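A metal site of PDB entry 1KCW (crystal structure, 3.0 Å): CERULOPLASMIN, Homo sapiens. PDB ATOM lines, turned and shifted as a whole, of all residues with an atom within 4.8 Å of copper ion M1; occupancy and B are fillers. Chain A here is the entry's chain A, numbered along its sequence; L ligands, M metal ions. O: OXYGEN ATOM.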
ATOM      1  N   HIS A 101      22.420  30.749 -29.882  1.00  0.00           N
ATOM      2  CA  HIS A 101      23.478  29.801 -29.569  1.00  0.00           C
ATOM      3  C   HIS A 101      23.614  28.896 -30.790  1.00  0.00           C
ATOM      4  O   HIS A 101      22.602  28.401 -31.290  1.00  0.00           O
ATOM      5  CB  HIS A 101      23.055  28.966 -28.371  1.00  0.00           C
ATOM      6  CG  HIS A 101      23.964  27.813 -28.086  1.00  0.00           C
ATOM      7  ND1 HIS A 101      25.335  27.916 -28.069  1.00  0.00           N
ATOM      8  CD2 HIS A 101      23.697  26.512 -27.847  1.00  0.00           C
ATOM      9  CE1 HIS A 101      25.845  26.696 -27.832  1.00  0.00           C
ATOM     10  NE2 HIS A 101      24.888  25.814 -27.684  1.00  0.00           N
ATOM     11  N   HIS A 103      25.462  25.462 -32.758  1.00  0.00           N
ATOM     12  CA  HIS A 103      25.931  24.194 -32.275  1.00  0.00           C
ATOM     13  C   HIS A 103      27.315  23.782 -32.698  1.00  0.00           C
ATOM     14  O   HIS A 103      28.129  23.465 -31.830  1.00  0.00           O
ATOM     15  CB  HIS A 103      24.971  23.059 -32.636  1.00  0.00           C
ATOM     16  CG  HIS A 103      24.070  22.633 -31.502  1.00  0.00           C
ATOM     17  ND1 HIS A 103      23.932  21.328 -31.092  1.00  0.00           N
ATOM     18  CD2 HIS A 103      23.134  23.332 -30.821  1.00  0.00           C
ATOM     19  CE1 HIS A 103      22.921  21.284 -30.209  1.00  0.00           C
ATOM     20  NE2 HIS A 103      22.397  22.479 -30.020  1.00  0.00           N
ATOM     21  N   HIS A 161      19.875  27.780 -32.211  1.00  0.00           N
ATOM     22  CA  HIS A 161      18.586  27.934 -31.548  1.00  0.00           C
ATOM     23  C   HIS A 161      18.755  28.844 -30.333  1.00  0.00           C
ATOM     24  O   HIS A 161      19.882  29.109 -29.905  1.00  0.00           O
ATOM     25  CB  HIS A 161      18.015  26.575 -31.112  1.00  0.00           C
ATOM     26  CG  HIS A 161      18.903  25.793 -30.198  1.00  0.00           C
ATOM     27  ND1 HIS A 161      18.715  25.699 -28.828  1.00  0.00           N
ATOM     28  CD2 HIS A 161      19.954  24.965 -30.468  1.00  0.00           C
ATOM     29  CE1 HIS A 161      19.623  24.828 -28.331  1.00  0.00           C
ATOM     30  NE2 HIS A 161      20.405  24.327 -29.277  1.00  0.00           N
ATOM     31  N   HIS A 978      24.901  16.305 -25.590  1.00  0.00           N
ATOM     32  CA  HIS A 978      25.438  17.479 -26.233  1.00  0.00           C
ATOM     33  C   HIS A 978      26.458  18.172 -25.347  1.00  0.00           C
ATOM     34  O   HIS A 978      26.221  18.301 -24.126  1.00  0.00           O
ATOM     35  CB  HIS A 978      24.338  18.457 -26.564  1.00  0.00           C
ATOM     36  CG  HIS A 978      24.822  19.676 -27.259  1.00  0.00           C
ATOM     37  ND1 HIS A 978      25.550  19.657 -28.431  1.00  0.00           N
ATOM     38  CD2 HIS A 978      24.697  20.982 -26.928  1.00  0.00           C
ATOM     39  CE1 HIS A 978      25.831  20.931 -28.759  1.00  0.00           C
ATOM     40  NE2 HIS A 978      25.330  21.782 -27.876  1.00  0.00           N
ATOM     41  N   HIS A 980      28.302  21.710 -24.951  1.00  0.00           N
ATOM     42  CA  HIS A 980      28.306  23.086 -25.450  1.00  0.00           C
ATOM     43  C   HIS A 980      29.727  23.576 -25.741  1.00  0.00           C
ATOM     44  O   HIS A 980      30.658  23.287 -25.011  1.00  0.00           O
ATOM     45  CB  HIS A 980      27.607  24.057 -24.455  1.00  0.00           C
ATOM     46  CG  HIS A 980      26.124  24.159 -24.635  1.00  0.00           C
ATOM     47  ND1 HIS A 980      25.239  24.439 -23.604  1.00  0.00           N
ATOM     48  CD2 HIS A 980      25.337  23.904 -25.715  1.00  0.00           C
ATOM     49  CE1 HIS A 980      23.987  24.323 -24.087  1.00  0.00           C
ATOM     50  NE2 HIS A 980      23.979  23.999 -25.366  1.00  0.00           N
ATOM     51  N   HIS A1020      24.749  18.401 -21.457  1.00  0.00           N
ATOM     52  CA  HIS A1020      23.398  17.948 -21.160  1.00  0.00           C
ATOM     53  C   HIS A1020      22.752  17.065 -22.214  1.00  0.00           C
ATOM     54  O   HIS A1020      23.254  16.953 -23.345  1.00  0.00           O
ATOM     55  CB  HIS A1020      22.483  19.152 -20.934  1.00  0.00           C
ATOM     56  CG  HIS A1020      22.390  20.090 -22.110  1.00  0.00           C
ATOM     57  ND1 HIS A1020      21.647  19.840 -23.242  1.00  0.00           N
ATOM     58  CD2 HIS A1020      22.903  21.331 -22.285  1.00  0.00           C
ATOM     59  CE1 HIS A1020      21.730  20.925 -24.038  1.00  0.00           C
ATOM     60  NE2 HIS A1020      22.486  21.862 -23.491  1.00  0.00           N
ATOM     61  N   HIS A1022      19.888  16.471 -24.752  1.00  0.00           N
ATOM     62  CA  HIS A1022      19.107  17.447 -25.505  1.00  0.00           C
ATOM     63  C   HIS A1022      17.609  17.158 -25.585  1.00  0.00           C
ATOM     64  O   HIS A1022      16.926  17.764 -26.407  1.00  0.00           O
ATOM     65  CB  HIS A1022      19.682  17.544 -26.923  1.00  0.00           C
ATOM     66  CG  HIS A1022      19.726  18.938 -27.495  1.00  0.00           C
ATOM     67  ND1 HIS A1022      18.625  19.734 -27.697  1.00  0.00           N
ATOM     68  CD2 HIS A1022      20.781  19.650 -27.963  1.00  0.00           C
ATOM     69  CE1 HIS A1022      19.028  20.888 -28.268  1.00  0.00           C
ATOM     70  NE2 HIS A1022      20.334  20.905 -28.462  1.00  0.00           N
HETATM   71  O     O L   1      21.940  23.268 -26.538  1.00  0.00           O
HETATM   72 CU    CU M   1      21.354  22.740 -28.225  1.00  0.00          CU
HETATM   73 CU    CU M   2      24.676  23.752 -27.963  1.00  0.00          CU
HETATM   74 CU    CU M   3      22.040  23.499 -24.708  1.00  0.00          CU
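An oxygen (O) of the ligand binds copper ion M1. NE2 of His 103 is bound to copper ion M1 (2.1 Å). A ring nitrogen (NE2) of His 1022 is bound to copper ion M1 (2.1 Å). Copper ion M1 is bound by NE2 of His 161 (2.1 Å).
The backbone carbonyl oxygen of His 101 is in hydrogen-bond range of the backbone NH of His 161. The backbone NH (N) of His 978 is in hydrogen-bond range of the backbone carbonyl oxygen (O) of His 1020 (2.9 Å).
Merely in contact with copper ion M1: His 978 (3.99 Å). Within 4 Å of copper ion M1: His 103, His 161, His 978 and His 1022. The nearest printed residue that does not touch copper ion M1 is His 980 (4.1 Å).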
